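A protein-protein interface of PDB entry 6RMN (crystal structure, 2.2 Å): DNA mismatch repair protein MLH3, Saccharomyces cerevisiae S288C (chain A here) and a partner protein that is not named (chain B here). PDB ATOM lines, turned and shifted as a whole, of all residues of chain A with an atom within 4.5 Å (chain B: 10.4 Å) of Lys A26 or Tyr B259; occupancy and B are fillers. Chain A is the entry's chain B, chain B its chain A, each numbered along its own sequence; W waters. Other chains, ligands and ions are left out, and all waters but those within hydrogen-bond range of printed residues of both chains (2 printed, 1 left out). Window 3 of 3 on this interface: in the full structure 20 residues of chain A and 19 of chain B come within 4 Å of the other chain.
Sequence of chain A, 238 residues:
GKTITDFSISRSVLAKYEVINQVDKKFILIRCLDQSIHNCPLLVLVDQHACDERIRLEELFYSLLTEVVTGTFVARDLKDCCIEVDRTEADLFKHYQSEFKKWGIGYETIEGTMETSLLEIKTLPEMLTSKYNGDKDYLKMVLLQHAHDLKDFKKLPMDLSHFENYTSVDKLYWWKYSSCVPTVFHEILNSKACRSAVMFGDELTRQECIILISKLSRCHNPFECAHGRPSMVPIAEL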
ATOM      1  N   GLN A  22     -19.610   5.002  17.216  1.00  0.00           N
ATOM      2  CA  GLN A  22     -20.451   6.165  17.484  1.00  0.00           C
ATOM      3  C   GLN A  22     -19.530   7.350  17.798  1.00  0.00           C
ATOM      4  O   GLN A  22     -18.495   7.185  18.452  1.00  0.00           O
ATOM      5  CB  GLN A  22     -21.428   5.893  18.642  1.00  0.00           C
ATOM      6  CG  GLN A  22     -22.542   6.938  18.779  1.00  0.00           C
ATOM      7  CD  GLN A  22     -23.389   6.787  20.024  1.00  0.00           C
ATOM      8  OE1 GLN A  22     -22.954   6.305  21.078  1.00  0.00           O
ATOM      9  NE2 GLN A  22     -24.629   7.223  19.932  1.00  0.00           N
ATOM     10  N   VAL A  23     -19.907   8.535  17.305  1.00  0.00           N
ATOM     11  CA  VAL A  23     -19.171   9.788  17.463  1.00  0.00           C
ATOM     12  C   VAL A  23     -20.118  10.826  18.075  1.00  0.00           C
ATOM     13  O   VAL A  23     -21.175  11.089  17.503  1.00  0.00           O
ATOM     14  CB  VAL A  23     -18.614  10.281  16.088  1.00  0.00           C
ATOM     15  CG1 VAL A  23     -18.077  11.710  16.170  1.00  0.00           C
ATOM     16  CG2 VAL A  23     -17.551   9.340  15.546  1.00  0.00           C
ATOM     17  N   ASP A  24     -19.733  11.404  19.235  1.00  0.00           N
ATOM     18  CA  ASP A  24     -20.415  12.493  19.956  1.00  0.00           C
ATOM     19  C   ASP A  24     -21.882  12.188  20.334  1.00  0.00           C
ATOM     20  O   ASP A  24     -22.644  13.115  20.622  1.00  0.00           O
ATOM     21  CB  ASP A  24     -20.299  13.800  19.127  1.00  0.00           C
ATOM     22  CG  ASP A  24     -20.649  15.086  19.847  1.00  0.00           C
ATOM     23  OD1 ASP A  24     -20.063  15.346  20.920  1.00  0.00           O
ATOM     24  OD2 ASP A  24     -21.500  15.839  19.331  1.00  0.00           O
ATOM     25  N   LYS A  25     -22.256  10.888  20.407  1.00  0.00           N
ATOM     26  CA  LYS A  25     -23.615  10.404  20.744  1.00  0.00           C
ATOM     27  C   LYS A  25     -24.666  10.899  19.719  1.00  0.00           C
ATOM     28  O   LYS A  25     -25.855  10.997  20.028  1.00  0.00           O
ATOM     29  CB  LYS A  25     -24.046  10.747  22.203  1.00  0.00           C
ATOM     30  CG  LYS A  25     -22.964  10.729  23.269  1.00  0.00           C
ATOM     31  CD  LYS A  25     -22.606   9.343  23.727  1.00  0.00           C
ATOM     32  CE  LYS A  25     -21.523   9.376  24.780  1.00  0.00           C
ATOM     33  NZ  LYS A  25     -20.166   9.462  24.186  1.00  0.00           N
ATOM     34  N   LYS A  26     -24.211  11.219  18.502  1.00  0.00           N
ATOM     35  CA  LYS A  26     -25.072  11.738  17.440  1.00  0.00           C
ATOM     36  C   LYS A  26     -24.837  11.027  16.111  1.00  0.00           C
ATOM     37  O   LYS A  26     -25.773  10.907  15.309  1.00  0.00           O
ATOM     38  CB  LYS A  26     -24.818  13.244  17.235  1.00  0.00           C
ATOM     39  CG  LYS A  26     -25.239  14.107  18.397  1.00  0.00           C
ATOM     40  CD  LYS A  26     -24.778  15.547  18.235  1.00  0.00           C
ATOM     41  CE  LYS A  26     -25.206  16.377  19.418  1.00  0.00           C
ATOM     42  NZ  LYS A  26     -24.502  15.969  20.669  1.00  0.00           N
ATOM     43  N   PHE A  27     -23.581  10.614  15.855  1.00  0.00           N
ATOM     44  CA  PHE A  27     -23.209  10.043  14.567  1.00  0.00           C
ATOM     45  C   PHE A  27     -22.640   8.667  14.604  1.00  0.00           C
ATOM     46  O   PHE A  27     -22.128   8.232  15.631  1.00  0.00           O
ATOM     47  CB  PHE A  27     -22.211  10.961  13.840  1.00  0.00           C
ATOM     48  CG  PHE A  27     -22.612  12.416  13.794  1.00  0.00           C
ATOM     49  CD1 PHE A  27     -23.628  12.848  12.947  1.00  0.00           C
ATOM     50  CD2 PHE A  27     -21.960  13.359  14.583  1.00  0.00           C
ATOM     51  CE1 PHE A  27     -24.002  14.192  12.913  1.00  0.00           C
ATOM     52  CE2 PHE A  27     -22.328  14.708  14.538  1.00  0.00           C
ATOM     53  CZ  PHE A  27     -23.346  15.115  13.702  1.00  0.00           C
ATOM     54  N   VAL A  46     -22.888   9.284   9.643  1.00  0.00           N
ATOM     55  CA  VAL A  46     -24.315   9.028   9.492  1.00  0.00           C
ATOM     56  C   VAL A  46     -25.054   9.581  10.720  1.00  0.00           C
ATOM     57  O   VAL A  46     -24.658   9.278  11.852  1.00  0.00           O
ATOM     58  CB  VAL A  46     -24.590   7.506   9.284  1.00  0.00           C
ATOM     59  CG1 VAL A  46     -26.078   7.226   9.099  1.00  0.00           C
ATOM     60  CG2 VAL A  46     -23.787   6.943   8.109  1.00  0.00           C
ATOM     61  N   ASP A  47     -26.133  10.376  10.498  1.00  0.00           N
ATOM     62  CA  ASP A  47     -27.002  10.878  11.567  1.00  0.00           C
ATOM     63  C   ASP A  47     -27.722   9.622  12.140  1.00  0.00           C
ATOM     64  O   ASP A  47     -28.399   8.913  11.385  1.00  0.00           O
ATOM     65  CB  ASP A  47     -28.007  11.876  10.966  1.00  0.00           C
ATOM     66  CG  ASP A  47     -29.033  12.503  11.912  1.00  0.00           C
ATOM     67  OD1 ASP A  47     -29.428  11.839  12.899  1.00  0.00           O
ATOM     68  OD2 ASP A  47     -29.482  13.633  11.634  1.00  0.00           O
ATOM     69  N   GLN A  48     -27.532   9.311  13.440  1.00  0.00           N
ATOM     70  CA  GLN A  48     -28.145   8.102  14.029  1.00  0.00           C
ATOM     71  C   GLN A  48     -29.680   8.149  14.086  1.00  0.00           C
ATOM     72  O   GLN A  48     -30.325   7.102  14.037  1.00  0.00           O
ATOM     73  CB  GLN A  48     -27.557   7.765  15.407  1.00  0.00           C
ATOM     74  CG  GLN A  48     -27.998   8.704  16.536  1.00  0.00           C
ATOM     75  CD  GLN A  48     -27.131   8.611  17.747  1.00  0.00           C
ATOM     76  OE1 GLN A  48     -25.924   8.381  17.664  1.00  0.00           O
ATOM     77  NE2 GLN A  48     -27.728   8.794  18.901  1.00  0.00           N
ATOM     78  N   PHE A 200     -30.586  12.080  19.297  1.00  0.00           N
ATOM     79  CA  PHE A 200     -29.280  12.661  19.542  1.00  0.00           C
ATOM     80  C   PHE A 200     -29.107  12.647  21.052  1.00  0.00           C
ATOM     81  O   PHE A 200     -30.054  12.962  21.789  1.00  0.00           O
ATOM     82  CB  PHE A 200     -29.214  14.097  18.995  1.00  0.00           C
ATOM     83  CG  PHE A 200     -28.832  14.231  17.536  1.00  0.00           C
ATOM     84  CD1 PHE A 200     -28.682  13.106  16.729  1.00  0.00           C
ATOM     85  CD2 PHE A 200     -28.577  15.479  16.980  1.00  0.00           C
ATOM     86  CE1 PHE A 200     -28.287  13.234  15.397  1.00  0.00           C
ATOM     87  CE2 PHE A 200     -28.196  15.605  15.639  1.00  0.00           C
ATOM     88  CZ  PHE A 200     -28.059  14.482  14.856  1.00  0.00           C
ATOM     89  N   ASN B  33     -10.777  11.510  23.151  1.00  0.00           N
ATOM     90  CA  ASN B  33     -11.884  10.569  23.249  1.00  0.00           C
ATOM     91  C   ASN B  33     -11.689   9.641  22.047  1.00  0.00           C
ATOM     92  O   ASN B  33     -11.833  10.069  20.900  1.00  0.00           O
ATOM     93  CB  ASN B  33     -13.239  11.288  23.238  1.00  0.00           C
ATOM     94  CG  ASN B  33     -14.378  10.394  23.643  1.00  0.00           C
ATOM     95  OD1 ASN B  33     -15.123   9.875  22.805  1.00  0.00           O
ATOM     96  ND2 ASN B  33     -14.528  10.184  24.942  1.00  0.00           N
ATOM     97  N   GLN B  48     -11.630  12.099  19.027  1.00  0.00           N
ATOM     98  CA  GLN B  48     -12.355  13.348  19.160  1.00  0.00           C
ATOM     99  C   GLN B  48     -11.666  14.160  20.250  1.00  0.00           C
ATOM    100  O   GLN B  48     -11.356  13.624  21.317  1.00  0.00           O
ATOM    101  CB  GLN B  48     -13.835  13.104  19.521  1.00  0.00           C
ATOM    102  CG  GLN B  48     -14.670  14.381  19.536  1.00  0.00           C
ATOM    103  CD  GLN B  48     -16.116  14.181  19.914  1.00  0.00           C
ATOM    104  OE1 GLN B  48     -16.717  13.126  19.692  1.00  0.00           O
ATOM    105  NE2 GLN B  48     -16.717  15.211  20.475  1.00  0.00           N
ATOM    106  N   HIS B  49     -11.408  15.443  19.965  1.00  0.00           N
ATOM    107  CA  HIS B  49     -10.861  16.404  20.924  1.00  0.00           C
ATOM    108  C   HIS B  49     -11.808  17.582  20.886  1.00  0.00           C
ATOM    109  O   HIS B  49     -11.958  18.216  19.835  1.00  0.00           O
ATOM    110  CB  HIS B  49      -9.417  16.830  20.607  1.00  0.00           C
ATOM    111  CG  HIS B  49      -8.926  17.922  21.518  1.00  0.00           C
ATOM    112  ND1 HIS B  49      -8.626  19.187  21.036  1.00  0.00           N
ATOM    113  CD2 HIS B  49      -8.745  17.912  22.860  1.00  0.00           C
ATOM    114  CE1 HIS B  49      -8.242  19.887  22.088  1.00  0.00           C
ATOM    115  NE2 HIS B  49      -8.310  19.166  23.209  1.00  0.00           N
ATOM    116  N   ASP B  50     -12.491  17.833  22.026  1.00  0.00           N
ATOM    117  CA  ASP B  50     -13.528  18.851  22.191  1.00  0.00           C
ATOM    118  C   ASP B  50     -14.659  18.507  21.237  1.00  0.00           C
ATOM    119  O   ASP B  50     -15.222  17.417  21.367  1.00  0.00           O
ATOM    120  CB  ASP B  50     -12.987  20.283  21.998  1.00  0.00           C
ATOM    121  CG  ASP B  50     -12.044  20.739  23.086  1.00  0.00           C
ATOM    122  OD1 ASP B  50     -12.115  20.179  24.208  1.00  0.00           O
ATOM    123  OD2 ASP B  50     -11.242  21.667  22.824  1.00  0.00           O
ATOM    124  N   LEU B  51     -14.943  19.377  20.246  1.00  0.00           N
ATOM    125  CA  LEU B  51     -15.980  19.113  19.248  1.00  0.00           C
ATOM    126  C   LEU B  51     -15.368  19.031  17.843  1.00  0.00           C
ATOM    127  O   LEU B  51     -15.964  19.480  16.859  1.00  0.00           O
ATOM    128  CB  LEU B  51     -17.132  20.130  19.335  1.00  0.00           C
ATOM    129  CG  LEU B  51     -17.874  20.231  20.674  1.00  0.00           C
ATOM    130  CD1 LEU B  51     -18.941  21.299  20.609  1.00  0.00           C
ATOM    131  CD2 LEU B  51     -18.484  18.888  21.096  1.00  0.00           C
ATOM    132  N   LYS B  52     -14.159  18.449  17.771  1.00  0.00           N
ATOM    133  CA  LYS B  52     -13.399  18.252  16.539  1.00  0.00           C
ATOM    134  C   LYS B  52     -12.985  16.802  16.421  1.00  0.00           C
ATOM    135  O   LYS B  52     -12.664  16.168  17.430  1.00  0.00           O
ATOM    136  CB  LYS B  52     -12.150  19.142  16.519  1.00  0.00           C
ATOM    137  CG  LYS B  52     -12.395  20.535  15.982  1.00  0.00           C
ATOM    138  CD  LYS B  52     -11.104  21.312  15.813  1.00  0.00           C
ATOM    139  CE  LYS B  52     -11.368  22.787  15.656  1.00  0.00           C
ATOM    140  NZ  LYS B  52     -11.760  23.415  16.944  1.00  0.00           N
ATOM    141  N   LEU B  53     -12.991  16.285  15.186  1.00  0.00           N
ATOM    142  CA  LEU B  53     -12.590  14.919  14.870  1.00  0.00           C
ATOM    143  C   LEU B  53     -11.223  14.927  14.178  1.00  0.00           C
ATOM    144  O   LEU B  53     -10.984  15.731  13.261  1.00  0.00           O
ATOM    145  CB  LEU B  53     -13.646  14.241  13.997  1.00  0.00           C
ATOM    146  CG  LEU B  53     -13.793  12.733  14.150  1.00  0.00           C
ATOM    147  CD1 LEU B  53     -14.328  12.375  15.533  1.00  0.00           C
ATOM    148  CD2 LEU B  53     -14.746  12.191  13.086  1.00  0.00           C
ATOM    149  N   ALA B 253     -12.933  16.671  10.733  1.00  0.00           N
ATOM    150  CA  ALA B 253     -14.262  17.260  10.885  1.00  0.00           C
ATOM    151  C   ALA B 253     -14.372  18.214  12.070  1.00  0.00           C
ATOM    152  O   ALA B 253     -13.781  17.970  13.122  1.00  0.00           O
ATOM    153  CB  ALA B 253     -15.313  16.169  11.010  1.00  0.00           C
ATOM    154  N   ASN B 254     -15.159  19.294  11.886  1.00  0.00           N
ATOM    155  CA  ASN B 254     -15.510  20.269  12.912  1.00  0.00           C
ATOM    156  C   ASN B 254     -17.006  20.035  13.146  1.00  0.00           C
ATOM    157  O   ASN B 254     -17.837  20.441  12.329  1.00  0.00           O
ATOM    158  CB  ASN B 254     -15.221  21.704  12.445  1.00  0.00           C
ATOM    159  CG  ASN B 254     -15.409  22.762  13.516  1.00  0.00           C
ATOM    160  OD1 ASN B 254     -15.032  22.587  14.682  1.00  0.00           O
ATOM    161  ND2 ASN B 254     -15.981  23.896  13.142  1.00  0.00           N
ATOM    162  N   LEU B 255     -17.332  19.306  14.233  1.00  0.00           N
ATOM    163  CA  LEU B 255     -18.692  18.897  14.611  1.00  0.00           C
ATOM    164  C   LEU B 255     -19.708  20.066  14.765  1.00  0.00           C
ATOM    165  O   LEU B 255     -20.843  19.838  14.351  1.00  0.00           O
ATOM    166  CB  LEU B 255     -18.709  17.981  15.851  1.00  0.00           C
ATOM    167  CG  LEU B 255     -17.776  16.742  15.819  1.00  0.00           C
ATOM    168  CD1 LEU B 255     -17.732  16.051  17.168  1.00  0.00           C
ATOM    169  CD2 LEU B 255     -18.155  15.755  14.714  1.00  0.00           C
ATOM    170  N   PRO B 256     -19.394  21.312  15.225  1.00  0.00           N
ATOM    171  CA  PRO B 256     -20.438  22.361  15.236  1.00  0.00           C
ATOM    172  C   PRO B 256     -20.997  22.678  13.839  1.00  0.00           C
ATOM    173  O   PRO B 256     -22.162  23.064  13.723  1.00  0.00           O
ATOM    174  CB  PRO B 256     -19.724  23.568  15.854  1.00  0.00           C
ATOM    175  CG  PRO B 256     -18.591  22.990  16.612  1.00  0.00           C
ATOM    176  CD  PRO B 256     -18.132  21.846  15.771  1.00  0.00           C
ATOM    177  N   ASP B 257     -20.181  22.467  12.780  1.00  0.00           N
ATOM    178  CA  ASP B 257     -20.582  22.658  11.384  1.00  0.00           C
ATOM    179  C   ASP B 257     -21.503  21.528  10.920  1.00  0.00           C
ATOM    180  O   ASP B 257     -22.322  21.729  10.027  1.00  0.00           O
ATOM    181  CB  ASP B 257     -19.352  22.769  10.464  1.00  0.00           C
ATOM    182  CG  ASP B 257     -18.446  23.967  10.734  1.00  0.00           C
ATOM    183  OD1 ASP B 257     -18.978  25.067  11.040  1.00  0.00           O
ATOM    184  OD2 ASP B 257     -17.210  23.813  10.613  1.00  0.00           O
ATOM    185  N   LEU B 258     -21.367  20.346  11.535  1.00  0.00           N
ATOM    186  CA  LEU B 258     -22.169  19.159  11.249  1.00  0.00           C
ATOM    187  C   LEU B 258     -23.522  19.227  11.952  1.00  0.00           C
ATOM    188  O   LEU B 258     -24.493  18.682  11.425  1.00  0.00           O
ATOM    189  CB  LEU B 258     -21.415  17.871  11.648  1.00  0.00           C
ATOM    190  CG  LEU B 258     -20.586  17.122  10.569  1.00  0.00           C
ATOM    191  CD1 LEU B 258     -21.464  16.594   9.424  1.00  0.00           C
ATOM    192  CD2 LEU B 258     -19.396  17.936  10.063  1.00  0.00           C
ATOM    193  N   TYR B 259     -23.598  19.914  13.123  1.00  0.00           N
ATOM    194  CA  TYR B 259     -24.848  20.094  13.876  1.00  0.00           C
ATOM    195  C   TYR B 259     -25.833  20.891  13.033  1.00  0.00           C
ATOM    196  O   TYR B 259     -27.019  20.591  13.059  1.00  0.00           O
ATOM    197  CB  TYR B 259     -24.630  20.831  15.216  1.00  0.00           C
ATOM    198  CG  TYR B 259     -23.656  20.202  16.192  1.00  0.00           C
ATOM    199  CD1 TYR B 259     -23.464  18.820  16.229  1.00  0.00           C
ATOM    200  CD2 TYR B 259     -22.996  20.975  17.141  1.00  0.00           C
ATOM    201  CE1 TYR B 259     -22.572  18.239  17.129  1.00  0.00           C
ATOM    202  CE2 TYR B 259     -22.104  20.406  18.048  1.00  0.00           C
ATOM    203  CZ  TYR B 259     -21.901  19.036  18.043  1.00  0.00           C
ATOM    204  OH  TYR B 259     -21.029  18.479  18.945  1.00  0.00           O
ATOM    205  N   LYS B 260     -25.321  21.899  12.286  1.00  0.00           N
ATOM    206  CA  LYS B 260     -26.048  22.776  11.363  1.00  0.00           C
ATOM    207  C   LYS B 260     -26.697  21.971  10.210  1.00  0.00           C
ATOM    208  O   LYS B 260     -27.821  22.288   9.815  1.00  0.00           O
ATOM    209  CB  LYS B 260     -25.083  23.843  10.803  1.00  0.00           C
ATOM    210  CG  LYS B 260     -25.750  24.974  10.023  1.00  0.00           C
ATOM    211  CD  LYS B 260     -24.723  25.854   9.326  1.00  0.00           C
ATOM    212  CE  LYS B 260     -25.367  27.034   8.641  1.00  0.00           C
ATOM    213  NZ  LYS B 260     -24.358  27.934   8.022  1.00  0.00           N
ATOM    214  N   VAL B 261     -25.991  20.939   9.682  1.00  0.00           N
ATOM    215  CA  VAL B 261     -26.456  20.059   8.590  1.00  0.00           C
ATOM    216  C   VAL B 261     -27.694  19.252   9.023  1.00  0.00           C
ATOM    217  O   VAL B 261     -28.646  19.116   8.250  1.00  0.00           O
ATOM    218  CB  VAL B 261     -25.331  19.130   8.043  1.00  0.00           C
ATOM    219  CG1 VAL B 261     -25.823  18.309   6.850  1.00  0.00           C
ATOM    220  CG2 VAL B 261     -24.078  19.922   7.666  1.00  0.00           C
ATOM    221  N   PHE B 262     -27.668  18.724  10.258  1.00  0.00           N
ATOM    222  CA  PHE B 262     -28.747  17.927  10.846  1.00  0.00           C
ATOM    223  C   PHE B 262     -29.432  18.700  11.996  1.00  0.00           C
ATOM    224  O   PHE B 262     -29.879  18.087  12.972  1.00  0.00           O
ATOM    225  CB  PHE B 262     -28.181  16.581  11.338  1.00  0.00           C
ATOM    226  CG  PHE B 262     -27.273  15.857  10.368  1.00  0.00           C
ATOM    227  CD1 PHE B 262     -27.795  15.173   9.275  1.00  0.00           C
ATOM    228  CD2 PHE B 262     -25.900  15.837  10.563  1.00  0.00           C
ATOM    229  CE1 PHE B 262     -26.954  14.496   8.387  1.00  0.00           C
ATOM    230  CE2 PHE B 262     -25.062  15.148   9.682  1.00  0.00           C
ATOM    231  CZ  PHE B 262     -25.596  14.477   8.603  1.00  0.00           C
ATOM    232  N   GLU B 263     -29.509  20.055  11.862  1.00  0.00           N
ATOM    233  CA  GLU B 263     -30.086  20.993  12.841  1.00  0.00           C
ATOM    234  C   GLU B 263     -31.533  20.659  13.187  1.00  0.00           C
ATOM    235  O   GLU B 263     -31.887  20.593  14.369  1.00  0.00           O
ATOM    236  CB  GLU B 263     -29.953  22.446  12.355  1.00  0.00           C
ATOM    237  CG  GLU B 263     -29.982  23.464  13.482  1.00  0.00           C
ATOM    238  CD  GLU B 263     -30.164  24.911  13.062  1.00  0.00           C
ATOM    239  OE1 GLU B 263     -29.355  25.407  12.244  1.00  0.00           O
ATOM    240  OE2 GLU B 263     -31.110  25.556  13.569  1.00  0.00           O
ATOM    241  N   ARG B 264     -32.357  20.448  12.152  1.00  0.00           N
ATOM    242  CA  ARG B 264     -33.762  20.083  12.285  1.00  0.00           C
ATOM    243  C   ARG B 264     -33.987  18.817  11.465  1.00  0.00           C
ATOM    244  O   ARG B 264     -33.201  18.537  10.553  1.00  0.00           O
ATOM    245  CB  ARG B 264     -34.680  21.236  11.835  1.00  0.00           C
ATOM    246  CG  ARG B 264     -34.694  22.425  12.802  1.00  0.00           C
ATOM    247  CD  ARG B 264     -35.863  23.354  12.532  1.00  0.00           C
ATOM    248  NE  ARG B 264     -35.991  24.393  13.557  1.00  0.00           N
ATOM    249  CZ  ARG B 264     -37.014  25.241  13.649  1.00  0.00           C
ATOM    250  NH1 ARG B 264     -37.045  26.151  14.614  1.00  0.00           N
ATOM    251  NH2 ARG B 264     -38.015  25.184  12.778  1.00  0.00           N
ATOM    252  N   CYS B 265     -35.006  18.020  11.827  1.00  0.00           N
ATOM    253  CA  CYS B 265     -35.318  16.766  11.131  1.00  0.00           C
ATOM    254  C   CYS B 265     -36.089  17.025   9.821  1.00  0.00           C
ATOM    255  O   CYS B 265     -36.654  18.127   9.653  1.00  0.00           O
ATOM    256  CB  CYS B 265     -36.063  15.801  12.053  1.00  0.00           C
ATOM    257  SG  CYS B 265     -36.079  14.083  11.478  1.00  0.00           S
ATOM    258  OXT CYS B 265     -36.101  16.139   8.942  1.00  0.00           O
HETATM  259  O   HOH W   1     -17.032  10.477  20.088  1.00  0.00           O
HETATM  260  O   HOH W   2     -17.374   8.798  24.886  1.00  0.00           O
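The side-chain amide nitrogen (NE2) of Gln B48 lies within hydrogen-bond range of the side-chain carboxylate (OD1) of Asp A24 (3.4 Å). The side-chain hydroxyl (OH) of Tyr B259 lies within hydrogen-bond range of the side-chain carboxylate (OD2) of Asp A24 (2.7 Å).
The side-chain carboxylate of Asp A24 is in salt-bridge range of the side-chain amino group of Lys A26, 3.3 Å away. The backbone NH (N) of Leu B255 is in hydrogen-bond range of the backbone carbonyl oxygen (O) of Leu B51, at 3.0 Å. The side-chain amide nitrogen (NE2) of Gln B48 sits at hydrogen-bond distance from the backbone carbonyl oxygen (O) of Asp B50 (2.8 Å). O of Asn B33 sits at hydrogen-bond distance from N of Gln B48 (2.8 Å). The backbone carbonyl oxygen (O) of Lys A26 lies within hydrogen-bond range of the backbone NH (N) of Gln A48 (3.0 Å). The backbone NH of Leu B53 is in hydrogen-bond range of the backbone carbonyl oxygen of Ala B253 (2.8 Å).
Among the printed residues, merely in contact across the chains: Asp A47 with Phe B262 (3.2 Å), Phe A27 with Phe B262 (3.4 Å), Lys A26 with Tyr B259 (3.7 Å), Val A23 with Leu B53 (3.9 Å), Asp A24 with Leu B51 (3.9 Å), Asp A24 with Leu B255 (3.9 Å) and Phe A27 with Leu B258 (3.9 Å).
Asp A24 touches just these residues of chain B: Gln B48, Leu B51, Leu B255 and Tyr B259. Of chain B, only Tyr B259 (3.7 Å) comes within 4 Å of Lys A26. Printed residues of chain B within 4 Å of Asp A47: Phe B262 (3.2 Å). No residue of chain B comes within 4 Å of Gln A48. Printed residues of chain A within 4 Å of Gln B48: Asp A24 (3.4 Å). Printed residues of chain A within 4 Å of Leu B51: Asp A24 (3.9 Å). Asp B257 touches none of the printed residues of chain A. Tyr B259 touches two residues of chain A. Printed residues of chain A within 4 Å of Phe B262: Phe A27 and Asp A47. The nearest residue of chain B that does not touch Lys A26 is Leu B51 (6.7 Å).
Of the 10 printed residues of chain A, 5 touch a printed residue of chain B. Hydrophobic or aromatic side chains of chain A within 4 Å of the printed part of chain B: Val A23 and Phe A27. Hydrophobic or aromatic side chains of chain B within 4 Å of the printed part of chain A: Leu B51, Leu B53, Leu B255, Leu B258, Tyr B259 and Phe B262. Along chain B the printed residues that touch a printed residue of chain A span positions 48 to 262. Among the printed residues, 9 pairs touch across the chains.
Water W1 lies within hydrogen-bond range of OE1 of Gln B48 (2.7 Å), N of Asp A24 (3.0 Å) and OD1 of Asn B33 (3.4 Å). Water W2 bridges the side-chain amino group of Lys A25 (3.0 Å) and the side-chain amide nitrogen of Asn B33 (3.2 Å).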
